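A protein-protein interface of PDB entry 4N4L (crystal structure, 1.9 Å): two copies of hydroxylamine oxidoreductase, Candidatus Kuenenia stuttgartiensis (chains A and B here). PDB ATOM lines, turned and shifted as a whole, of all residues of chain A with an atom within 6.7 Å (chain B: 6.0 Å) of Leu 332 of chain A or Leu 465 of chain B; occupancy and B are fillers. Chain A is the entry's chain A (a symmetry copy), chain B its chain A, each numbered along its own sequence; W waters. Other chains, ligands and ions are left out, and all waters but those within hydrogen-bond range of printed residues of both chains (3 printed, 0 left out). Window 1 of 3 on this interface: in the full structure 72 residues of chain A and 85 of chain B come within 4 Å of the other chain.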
ATOM      1  N   GLN A 291     -39.502  -5.386 -24.063  1.00  0.00           N
ATOM      2  CA  GLN A 291     -39.581  -3.957 -24.291  1.00  0.00           C
ATOM      3  C   GLN A 291     -40.997  -3.529 -24.625  1.00  0.00           C
ATOM      4  O   GLN A 291     -41.627  -4.066 -25.545  1.00  0.00           O
ATOM      5  CB  GLN A 291     -38.647  -3.551 -25.431  1.00  0.00           C
ATOM      6  CG  GLN A 291     -38.624  -2.051 -25.710  1.00  0.00           C
ATOM      7  CD  GLN A 291     -37.602  -1.662 -26.760  1.00  0.00           C
ATOM      8  OE1 GLN A 291     -37.044  -2.516 -27.451  1.00  0.00           O
ATOM      9  NE2 GLN A 291     -37.363  -0.360 -26.895  1.00  0.00           N
ATOM     10  N   ASP A 327     -40.137   6.058 -20.395  1.00  0.00           N
ATOM     11  CA  ASP A 327     -40.353   5.487 -21.730  1.00  0.00           C
ATOM     12  C   ASP A 327     -39.115   5.678 -22.605  1.00  0.00           C
ATOM     13  O   ASP A 327     -38.642   4.733 -23.234  1.00  0.00           O
ATOM     14  CB  ASP A 327     -41.548   6.128 -22.429  1.00  0.00           C
ATOM     15  CG  ASP A 327     -42.835   6.008 -21.640  1.00  0.00           C
ATOM     16  OD1 ASP A 327     -43.002   5.020 -20.896  1.00  0.00           O
ATOM     17  OD2 ASP A 327     -43.687   6.916 -21.772  1.00  0.00           O
ATOM     18  N   ALA A 328     -38.600   6.905 -22.635  1.00  0.00           N
ATOM     19  CA  ALA A 328     -37.440   7.236 -23.464  1.00  0.00           C
ATOM     20  C   ALA A 328     -36.180   6.505 -23.004  1.00  0.00           C
ATOM     21  O   ALA A 328     -35.431   5.968 -23.822  1.00  0.00           O
ATOM     22  CB  ALA A 328     -37.209   8.755 -23.473  1.00  0.00           C
ATOM     23  N   GLY A 329     -35.947   6.480 -21.693  1.00  0.00           N
ATOM     24  CA  GLY A 329     -34.766   5.836 -21.137  1.00  0.00           C
ATOM     25  C   GLY A 329     -34.769   4.339 -21.355  1.00  0.00           C
ATOM     26  O   GLY A 329     -33.738   3.746 -21.660  1.00  0.00           O
ATOM     27  N   VAL A 330     -35.933   3.723 -21.194  1.00  0.00           N
ATOM     28  CA  VAL A 330     -36.077   2.303 -21.482  1.00  0.00           C
ATOM     29  C   VAL A 330     -35.784   2.010 -22.963  1.00  0.00           C
ATOM     30  O   VAL A 330     -35.027   1.094 -23.278  1.00  0.00           O
ATOM     31  CB  VAL A 330     -37.475   1.781 -21.078  1.00  0.00           C
ATOM     32  CG1 VAL A 330     -37.740   0.415 -21.705  1.00  0.00           C
ATOM     33  CG2 VAL A 330     -37.586   1.702 -19.556  1.00  0.00           C
ATOM     34  N   ASN A 331     -36.342   2.809 -23.867  1.00  0.00           N
ATOM     35  CA  ASN A 331     -36.164   2.556 -25.302  1.00  0.00           C
ATOM     36  C   ASN A 331     -34.702   2.687 -25.732  1.00  0.00           C
ATOM     37  O   ASN A 331     -34.218   1.903 -26.554  1.00  0.00           O
ATOM     38  CB  ASN A 331     -37.082   3.455 -26.131  1.00  0.00           C
ATOM     39  CG  ASN A 331     -38.548   3.049 -26.026  1.00  0.00           C
ATOM     40  OD1 ASN A 331     -38.870   1.909 -25.673  1.00  0.00           O
ATOM     41  ND2 ASN A 331     -39.440   3.971 -26.352  1.00  0.00           N
ATOM     42  N   LEU A 332     -33.986   3.645 -25.153  1.00  0.00           N
ATOM     43  CA  LEU A 332     -32.550   3.769 -25.414  1.00  0.00           C
ATOM     44  C   LEU A 332     -31.796   2.541 -24.885  1.00  0.00           C
ATOM     45  O   LEU A 332     -30.915   2.012 -25.567  1.00  0.00           O
ATOM     46  CB  LEU A 332     -32.001   5.072 -24.818  1.00  0.00           C
ATOM     47  CG  LEU A 332     -30.553   5.492 -25.130  1.00  0.00           C
ATOM     48  CD1 LEU A 332     -29.547   4.676 -24.330  1.00  0.00           C
ATOM     49  CD2 LEU A 332     -30.234   5.432 -26.640  1.00  0.00           C
ATOM     50  N   SER A 333     -32.173   2.064 -23.696  1.00  0.00           N
ATOM     51  CA  SER A 333     -31.486   0.934 -23.065  1.00  0.00           C
ATOM     52  C   SER A 333     -31.504  -0.335 -23.921  1.00  0.00           C
ATOM     53  O   SER A 333     -30.567  -1.130 -23.873  1.00  0.00           O
ATOM     54  CB  SER A 333     -32.074   0.634 -21.677  1.00  0.00           C
ATOM     55  OG  SER A 333     -33.303  -0.063 -21.759  1.00  0.00           O
ATOM     56  N   PHE A 334     -32.563  -0.525 -24.703  1.00  0.00           N
ATOM     57  CA  PHE A 334     -32.669  -1.720 -25.536  1.00  0.00           C
ATOM     58  C   PHE A 334     -31.754  -1.734 -26.763  1.00  0.00           C
ATOM     59  O   PHE A 334     -31.490  -2.808 -27.305  1.00  0.00           O
ATOM     60  CB  PHE A 334     -34.121  -1.994 -25.920  1.00  0.00           C
ATOM     61  CG  PHE A 334     -34.843  -2.816 -24.903  1.00  0.00           C
ATOM     62  CD1 PHE A 334     -34.752  -4.194 -24.932  1.00  0.00           C
ATOM     63  CD2 PHE A 334     -35.572  -2.217 -23.887  1.00  0.00           C
ATOM     64  CE1 PHE A 334     -35.389  -4.968 -23.985  1.00  0.00           C
ATOM     65  CE2 PHE A 334     -36.223  -2.987 -22.938  1.00  0.00           C
ATOM     66  CZ  PHE A 334     -36.126  -4.364 -22.984  1.00  0.00           C
ATOM     67  N   THR A 335     -31.244  -0.573 -27.176  1.00  0.00           N
ATOM     68  CA  THR A 335     -30.261  -0.529 -28.267  1.00  0.00           C
ATOM     69  C   THR A 335     -28.972  -1.243 -27.867  1.00  0.00           C
ATOM     70  O   THR A 335     -28.355  -1.931 -28.678  1.00  0.00           O
ATOM     71  CB  THR A 335     -29.939   0.917 -28.731  1.00  0.00           C
ATOM     72  OG1 THR A 335     -29.277   1.643 -27.686  1.00  0.00           O
ATOM     73  CG2 THR A 335     -31.210   1.645 -29.156  1.00  0.00           C
ATOM     74  N   LYS A 336     -28.592  -1.105 -26.601  1.00  0.00           N
ATOM     75  CA  LYS A 336     -27.392  -1.742 -26.085  1.00  0.00           C
ATOM     76  C   LYS A 336     -27.592  -3.250 -25.935  1.00  0.00           C
ATOM     77  O   LYS A 336     -26.669  -4.033 -26.173  1.00  0.00           O
ATOM     78  CB  LYS A 336     -27.003  -1.124 -24.739  1.00  0.00           C
ATOM     79  CG  LYS A 336     -26.685   0.367 -24.795  1.00  0.00           C
ATOM     80  CD  LYS A 336     -26.458   0.931 -23.390  1.00  0.00           C
ATOM     81  CE  LYS A 336     -26.378   2.454 -23.393  1.00  0.00           C
ATOM     82  NZ  LYS A 336     -26.265   2.986 -22.001  1.00  0.00           N
ATOM     83  N   TRP A 337     -28.797  -3.664 -25.545  1.00  0.00           N
ATOM     84  CA  TRP A 337     -29.097  -5.091 -25.454  1.00  0.00           C
ATOM     85  C   TRP A 337     -29.076  -5.733 -26.844  1.00  0.00           C
ATOM     86  O   TRP A 337     -28.522  -6.815 -27.022  1.00  0.00           O
ATOM     87  CB  TRP A 337     -30.444  -5.335 -24.764  1.00  0.00           C
ATOM     88  CG  TRP A 337     -31.038  -6.690 -25.035  1.00  0.00           C
ATOM     89  CD1 TRP A 337     -32.266  -6.942 -25.557  1.00  0.00           C
ATOM     90  CD2 TRP A 337     -30.428  -7.969 -24.804  1.00  0.00           C
ATOM     91  NE1 TRP A 337     -32.469  -8.296 -25.666  1.00  0.00           N
ATOM     92  CE2 TRP A 337     -31.356  -8.949 -25.212  1.00  0.00           C
ATOM     93  CE3 TRP A 337     -29.194  -8.381 -24.288  1.00  0.00           C
ATOM     94  CZ2 TRP A 337     -31.088 -10.319 -25.121  1.00  0.00           C
ATOM     95  CZ3 TRP A 337     -28.925  -9.743 -24.202  1.00  0.00           C
ATOM     96  CH2 TRP A 337     -29.872 -10.697 -24.615  1.00  0.00           C
ATOM     97  N   ARG A 338     -29.680  -5.070 -27.823  1.00  0.00           N
ATOM     98  CA  ARG A 338     -29.702  -5.613 -29.181  1.00  0.00           C
ATOM     99  C   ARG A 338     -28.290  -5.707 -29.770  1.00  0.00           C
ATOM    100  O   ARG A 338     -27.963  -6.691 -30.430  1.00  0.00           O
ATOM    101  CB  ARG A 338     -30.660  -4.830 -30.086  1.00  0.00           C
ATOM    102  CG  ARG A 338     -32.133  -5.143 -29.811  1.00  0.00           C
ATOM    103  CD  ARG A 338     -33.046  -4.529 -30.847  1.00  0.00           C
ATOM    104  NE  ARG A 338     -33.072  -3.069 -30.774  1.00  0.00           N
ATOM    105  CZ  ARG A 338     -33.915  -2.347 -30.034  1.00  0.00           C
ATOM    106  NH1 ARG A 338     -34.843  -2.926 -29.272  1.00  0.00           N
ATOM    107  NH2 ARG A 338     -33.832  -1.025 -30.067  1.00  0.00           N
ATOM    108  N   ALA A 420     -27.699   2.694 -17.148  1.00  0.00           N
ATOM    109  CA  ALA A 420     -27.163   2.913 -18.488  1.00  0.00           C
ATOM    110  C   ALA A 420     -25.666   2.644 -18.538  1.00  0.00           C
ATOM    111  O   ALA A 420     -25.186   1.979 -19.448  1.00  0.00           O
ATOM    112  CB  ALA A 420     -27.442   4.336 -18.941  1.00  0.00           C
ATOM    113  N   GLN A 423     -24.735  -0.963 -18.207  1.00  0.00           N
ATOM    114  CA  GLN A 423     -24.964  -1.571 -19.527  1.00  0.00           C
ATOM    115  C   GLN A 423     -23.769  -1.338 -20.446  1.00  0.00           C
ATOM    116  O   GLN A 423     -23.324  -2.257 -21.148  1.00  0.00           O
ATOM    117  CB  GLN A 423     -26.204  -0.993 -20.208  1.00  0.00           C
ATOM    118  CG  GLN A 423     -27.526  -1.579 -19.765  1.00  0.00           C
ATOM    119  CD  GLN A 423     -28.660  -1.082 -20.633  1.00  0.00           C
ATOM    120  OE1 GLN A 423     -28.886   0.124 -20.740  1.00  0.00           O
ATOM    121  NE2 GLN A 423     -29.359  -2.005 -21.285  1.00  0.00           N
ATOM    122  N   ASP B  20     -40.158   1.011 -31.582  1.00  0.00           N
ATOM    123  CA  ASP B  20     -40.163   0.789 -30.136  1.00  0.00           C
ATOM    124  C   ASP B  20     -41.304   1.507 -29.419  1.00  0.00           C
ATOM    125  O   ASP B  20     -41.797   1.027 -28.398  1.00  0.00           O
ATOM    126  CB  ASP B  20     -38.812   1.174 -29.511  1.00  0.00           C
ATOM    127  CG  ASP B  20     -38.389   2.619 -29.800  1.00  0.00           C
ATOM    128  OD1 ASP B  20     -37.221   2.946 -29.490  1.00  0.00           O
ATOM    129  OD2 ASP B  20     -39.186   3.427 -30.330  1.00  0.00           O
ATOM    130  N   TYR B  34     -35.290   1.430 -32.819  1.00  0.00           N
ATOM    131  CA  TYR B  34     -35.112   2.637 -32.031  1.00  0.00           C
ATOM    132  C   TYR B  34     -35.711   3.830 -32.757  1.00  0.00           C
ATOM    133  O   TYR B  34     -35.503   4.001 -33.963  1.00  0.00           O
ATOM    134  CB  TYR B  34     -33.633   2.898 -31.760  1.00  0.00           C
ATOM    135  CG  TYR B  34     -33.350   4.240 -31.122  1.00  0.00           C
ATOM    136  CD1 TYR B  34     -33.520   4.436 -29.749  1.00  0.00           C
ATOM    137  CD2 TYR B  34     -32.903   5.312 -31.889  1.00  0.00           C
ATOM    138  CE1 TYR B  34     -33.251   5.670 -29.165  1.00  0.00           C
ATOM    139  CE2 TYR B  34     -32.636   6.540 -31.321  1.00  0.00           C
ATOM    140  CZ  TYR B  34     -32.807   6.716 -29.960  1.00  0.00           C
ATOM    141  OH  TYR B  34     -32.534   7.946 -29.414  1.00  0.00           O
ATOM    142  N   PRO B 180     -26.724  10.155 -26.051  1.00  0.00           N
ATOM    143  CA  PRO B 180     -28.083  10.589 -26.380  1.00  0.00           C
ATOM    144  C   PRO B 180     -28.795  11.136 -25.148  1.00  0.00           C
ATOM    145  O   PRO B 180     -28.628  10.597 -24.048  1.00  0.00           O
ATOM    146  CB  PRO B 180     -28.761   9.312 -26.881  1.00  0.00           C
ATOM    147  CG  PRO B 180     -27.650   8.434 -27.324  1.00  0.00           C
ATOM    148  CD  PRO B 180     -26.482   8.756 -26.439  1.00  0.00           C
ATOM    149  N   GLU B 182     -31.748  11.204 -23.745  1.00  0.00           N
ATOM    150  CA  GLU B 182     -32.612  10.382 -22.883  1.00  0.00           C
ATOM    151  C   GLU B 182     -31.848   9.387 -22.008  1.00  0.00           C
ATOM    152  O   GLU B 182     -32.396   8.871 -21.033  1.00  0.00           O
ATOM    153  CB  GLU B 182     -33.680   9.642 -23.696  1.00  0.00           C
ATOM    154  CG  GLU B 182     -33.164   8.510 -24.591  1.00  0.00           C
ATOM    155  CD  GLU B 182     -32.919   8.937 -26.016  1.00  0.00           C
ATOM    156  OE1 GLU B 182     -33.169   8.112 -26.924  1.00  0.00           O
ATOM    157  OE2 GLU B 182     -32.478  10.092 -26.225  1.00  0.00           O
ATOM    158  N   GLU B 183     -30.597   9.104 -22.361  1.00  0.00           N
ATOM    159  CA  GLU B 183     -29.759   8.218 -21.560  1.00  0.00           C
ATOM    160  C   GLU B 183     -29.285   8.893 -20.270  1.00  0.00           C
ATOM    161  O   GLU B 183     -29.041   8.220 -19.260  1.00  0.00           O
ATOM    162  CB  GLU B 183     -28.547   7.764 -22.367  1.00  0.00           C
ATOM    163  CG  GLU B 183     -27.699   6.710 -21.674  1.00  0.00           C
ATOM    164  CD  GLU B 183     -26.454   6.344 -22.454  1.00  0.00           C
ATOM    165  OE1 GLU B 183     -25.635   5.579 -21.906  1.00  0.00           O
ATOM    166  OE2 GLU B 183     -26.299   6.811 -23.604  1.00  0.00           O
ATOM    167  N   GLY B 460     -22.755  -0.317 -34.363  1.00  0.00           N
ATOM    168  CA  GLY B 460     -23.814  -1.035 -33.678  1.00  0.00           C
ATOM    169  C   GLY B 460     -24.971  -0.080 -33.469  1.00  0.00           C
ATOM    170  O   GLY B 460     -24.833   1.124 -33.678  1.00  0.00           O
ATOM    171  N   GLU B 461     -26.113  -0.603 -33.045  1.00  0.00           N
ATOM    172  CA  GLU B 461     -27.311   0.217 -32.918  1.00  0.00           C
ATOM    173  C   GLU B 461     -27.147   1.365 -31.926  1.00  0.00           C
ATOM    174  O   GLU B 461     -27.679   2.452 -32.159  1.00  0.00           O
ATOM    175  CB  GLU B 461     -28.525  -0.638 -32.540  1.00  0.00           C
ATOM    176  CG  GLU B 461     -29.833   0.123 -32.655  1.00  0.00           C
ATOM    177  CD  GLU B 461     -31.051  -0.724 -32.357  1.00  0.00           C
ATOM    178  OE1 GLU B 461     -30.913  -1.947 -32.155  1.00  0.00           O
ATOM    179  OE2 GLU B 461     -32.161  -0.160 -32.342  1.00  0.00           O
ATOM    180  N   TYR B 462     -26.433   1.127 -30.823  1.00  0.00           N
ATOM    181  CA  TYR B 462     -26.146   2.199 -29.872  1.00  0.00           C
ATOM    182  C   TYR B 462     -24.964   3.057 -30.328  1.00  0.00           C
ATOM    183  O   TYR B 462     -25.057   4.286 -30.332  1.00  0.00           O
ATOM    184  CB  TYR B 462     -25.875   1.666 -28.461  1.00  0.00           C
ATOM    185  CG  TYR B 462     -25.474   2.772 -27.510  1.00  0.00           C
ATOM    186  CD1 TYR B 462     -26.420   3.671 -27.016  1.00  0.00           C
ATOM    187  CD2 TYR B 462     -24.142   2.951 -27.142  1.00  0.00           C
ATOM    188  CE1 TYR B 462     -26.053   4.703 -26.169  1.00  0.00           C
ATOM    189  CE2 TYR B 462     -23.767   3.978 -26.290  1.00  0.00           C
ATOM    190  CZ  TYR B 462     -24.724   4.852 -25.808  1.00  0.00           C
ATOM    191  OH  TYR B 462     -24.351   5.869 -24.964  1.00  0.00           O
ATOM    192  N   LEU B 463     -23.850   2.421 -30.685  1.00  0.00           N
ATOM    193  CA  LEU B 463     -22.648   3.169 -31.102  1.00  0.00           C
ATOM    194  C   LEU B 463     -22.937   4.145 -32.238  1.00  0.00           C
ATOM    195  O   LEU B 463     -22.384   5.249 -32.262  1.00  0.00           O
ATOM    196  CB  LEU B 463     -21.515   2.231 -31.521  1.00  0.00           C
ATOM    197  CG  LEU B 463     -20.859   1.393 -30.426  1.00  0.00           C
ATOM    198  CD1 LEU B 463     -19.728   0.551 -31.024  1.00  0.00           C
ATOM    199  CD2 LEU B 463     -20.350   2.267 -29.281  1.00  0.00           C
ATOM    200  N   ASP B 464     -23.811   3.749 -33.162  1.00  0.00           N
ATOM    201  CA  ASP B 464     -24.164   4.608 -34.295  1.00  0.00           C
ATOM    202  C   ASP B 464     -24.923   5.874 -33.884  1.00  0.00           C
ATOM    203  O   ASP B 464     -24.998   6.811 -34.669  1.00  0.00           O
ATOM    204  CB  ASP B 464     -24.981   3.838 -35.341  1.00  0.00           C
ATOM    205  CG  ASP B 464     -24.175   2.763 -36.052  1.00  0.00           C
ATOM    206  OD1 ASP B 464     -24.783   2.018 -36.844  1.00  0.00           O
ATOM    207  OD2 ASP B 464     -22.952   2.646 -35.814  1.00  0.00           O
ATOM    208  N   LEU B 465     -25.480   5.909 -32.668  1.00  0.00           N
ATOM    209  CA  LEU B 465     -26.197   7.096 -32.181  1.00  0.00           C
ATOM    210  C   LEU B 465     -25.274   8.164 -31.606  1.00  0.00           C
ATOM    211  O   LEU B 465     -25.718   9.280 -31.335  1.00  0.00           O
ATOM    212  CB  LEU B 465     -27.217   6.720 -31.097  1.00  0.00           C
ATOM    213  CG  LEU B 465     -28.324   5.731 -31.464  1.00  0.00           C
ATOM    214  CD1 LEU B 465     -29.169   5.422 -30.227  1.00  0.00           C
ATOM    215  CD2 LEU B 465     -29.203   6.259 -32.591  1.00  0.00           C
ATOM    216  N   LEU B 466     -24.001   7.833 -31.408  1.00  0.00           N
ATOM    217  CA  LEU B 466     -23.108   8.715 -30.660  1.00  0.00           C
ATOM    218  C   LEU B 466     -22.775   9.976 -31.453  1.00  0.00           C
ATOM    219  O   LEU B 466     -22.642   9.926 -32.675  1.00  0.00           O
ATOM    220  CB  LEU B 466     -21.836   7.973 -30.251  1.00  0.00           C
ATOM    221  CG  LEU B 466     -22.051   6.754 -29.345  1.00  0.00           C
ATOM    222  CD1 LEU B 466     -20.731   6.066 -29.041  1.00  0.00           C
ATOM    223  CD2 LEU B 466     -22.767   7.149 -28.052  1.00  0.00           C
ATOM    224  N   PRO B 467     -22.633  11.115 -30.757  1.00  0.00           N
ATOM    225  CA  PRO B 467     -22.433  12.398 -31.419  1.00  0.00           C
ATOM    226  C   PRO B 467     -21.066  12.564 -32.094  1.00  0.00           C
ATOM    227  O   PRO B 467     -20.932  13.400 -32.983  1.00  0.00           O
ATOM    228  CB  PRO B 467     -22.608  13.404 -30.277  1.00  0.00           C
ATOM    229  CG  PRO B 467     -22.153  12.683 -29.090  1.00  0.00           C
ATOM    230  CD  PRO B 467     -22.600  11.255 -29.292  1.00  0.00           C
ATOM    231  N   TRP B 469     -19.711  10.893 -34.342  1.00  0.00           N
ATOM    232  CA  TRP B 469     -19.872  10.685 -35.780  1.00  0.00           C
ATOM    233  C   TRP B 469     -20.197  11.960 -36.552  1.00  0.00           C
ATOM    234  O   TRP B 469     -19.844  12.079 -37.728  1.00  0.00           O
ATOM    235  CB  TRP B 469     -20.995   9.679 -36.047  1.00  0.00           C
ATOM    236  CG  TRP B 469     -20.693   8.305 -35.583  1.00  0.00           C
ATOM    237  CD1 TRP B 469     -21.299   7.628 -34.561  1.00  0.00           C
ATOM    238  CD2 TRP B 469     -19.714   7.421 -36.126  1.00  0.00           C
ATOM    239  NE1 TRP B 469     -20.755   6.376 -34.437  1.00  0.00           N
ATOM    240  CE2 TRP B 469     -19.778   6.223 -35.385  1.00  0.00           C
ATOM    241  CE3 TRP B 469     -18.786   7.524 -37.171  1.00  0.00           C
ATOM    242  CZ2 TRP B 469     -18.949   5.135 -35.652  1.00  0.00           C
ATOM    243  CZ3 TRP B 469     -17.964   6.447 -37.436  1.00  0.00           C
ATOM    244  CH2 TRP B 469     -18.050   5.266 -36.680  1.00  0.00           C
HETATM  245  O   HOH W   1     -35.457   6.609 -26.487  1.00  0.00           O
HETATM  246  O   HOH W   2     -37.410   6.011 -28.144  1.00  0.00           O
HETATM  247  O   HOH W   3     -35.548   1.000 -28.680  1.00  0.00           O
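OE1 of Glu 183 of chain B is in salt-bridge range of NZ of Lys 336 of chain A.
The side-chain carboxylate of Glu 461 of chain B lies within salt-bridge range of the guanidinium group of Arg 338 of chain A.
The side-chain amino group (NZ) of Lys 336 of chain A is in hydrogen-bond range of the backbone carbonyl oxygen (O) of Ala 420 of chain A.
The side-chain carboxylate (OE2) of Glu 183 of chain B is in hydrogen-bond range of the side-chain hydroxyl (OH) of Tyr 462 of chain B (2.6 Å).
OE1 of Glu 182 of chain B sits at hydrogen-bond distance from OH of Tyr 34 of chain B (2.6 Å).
The side-chain amide nitrogen (NE2) of Gln 291 of chain A sits at hydrogen-bond distance from the side-chain amide oxygen (OD1) of Asn 331 of chain A, at 3.0 Å.
The side-chain amide nitrogen (ND2) of Asn 331 of chain A sits close to the backbone carbonyl oxygen (O) of Asp 327 of chain A, 3.3 Å away.
The backbone carbonyl oxygen (O) of Leu 332 of chain A lies within hydrogen-bond range of the side-chain hydroxyl (OG1) of Thr 335 of chain A, at 2.7 Å.
CG of Glu 182 of chain B touches O of Ala 328 of chain A, 3.5 Å away.
CA of Gly 329 of chain A touches O of Glu 182 of chain B, at 3.9 Å.
Asp 20 of chain B touches Asn 331 of chain A.
CB of Leu 332 of chain A touches CG of Glu 182 of chain B, at 3.6 Å.
CE1 of Tyr 462 of chain B touches CD1 of Leu 332 of chain A, at 3.9 Å.
CD2 of Leu 332 of chain A touches CD1 of Leu 465 of chain B (3.7 Å).
Thr 335 of chain A touches Glu 461 of chain B.
OG1 of Thr 335 of chain A touches CB of Tyr 462 of chain B, at 3.5 Å.
Tyr 462 of chain B touches Lys 336 of chain A (CE1 to CE, 3.6 Å).
CB of Ala 420 of chain A touches CG of Glu 183 of chain B (3.6 Å).
Of the printed residues of chain B, Leu 332 of chain A touches Tyr 34 (3.9 Å), Glu 182 (3.6 Å), Glu 183 (3.8 Å), Tyr 462 (3.9 Å) and Leu 465 (3.7 Å).
Of chain A, only Leu 332 (3.7 Å) comes within 4 Å of Leu 465 of chain B.
Of the printed residues of chain B, Lys 336 of chain A touches Glu 183 (2.7 Å) and Tyr 462 (3.6 Å).
Of the printed residues of chain B, Arg 338 of chain A touches Tyr 34 (3.97 Å) and Glu 461 (2.8 Å).
Printed residues of chain B within 4 Å of Asn 331 of chain A: Asp 20.
Of the printed residues of chain A, Asp 20 of chain B touches Gln 291 (3.4 Å) and Asn 331 (3.4 Å).
Gly 460 of chain B touches none of the printed residues of chain A.
Asp 327 of chain A touches none of the printed residues of chain B.
The nearest printed residue of chain A that does not touch Glu 461 of chain B is Phe 334 of chain A (5.0 Å).
Hydrophobic or aromatic side chains of chain B that line the printed part of chain A: Tyr 34, Tyr 462 and Leu 465.
No position is printed for both chains.
Of the 17 pairs that touch across the chains among the printed residues, none has its exchanged pair printed and touching as well.
Water W3 lies within hydrogen-bond range of the backbone carbonyl oxygen (O) of Asn 331 of chain A, the side-chain carboxylate (OD1) of Asp 20 of chain B, the side-chain amide nitrogen (NE2) of Gln 291 of chain A and the guanidinium group (NH2) of Arg 338 of chain A.
Water W1 bridges the backbone carbonyl oxygen of Ala 328 of chain A and the side-chain carboxylate of Glu 182 of chain B.
Water W2 bridges OD1 of Asp 20 of chain B (3.4 Å) and ND2 of Asn 331 of chain A (3.4 Å).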
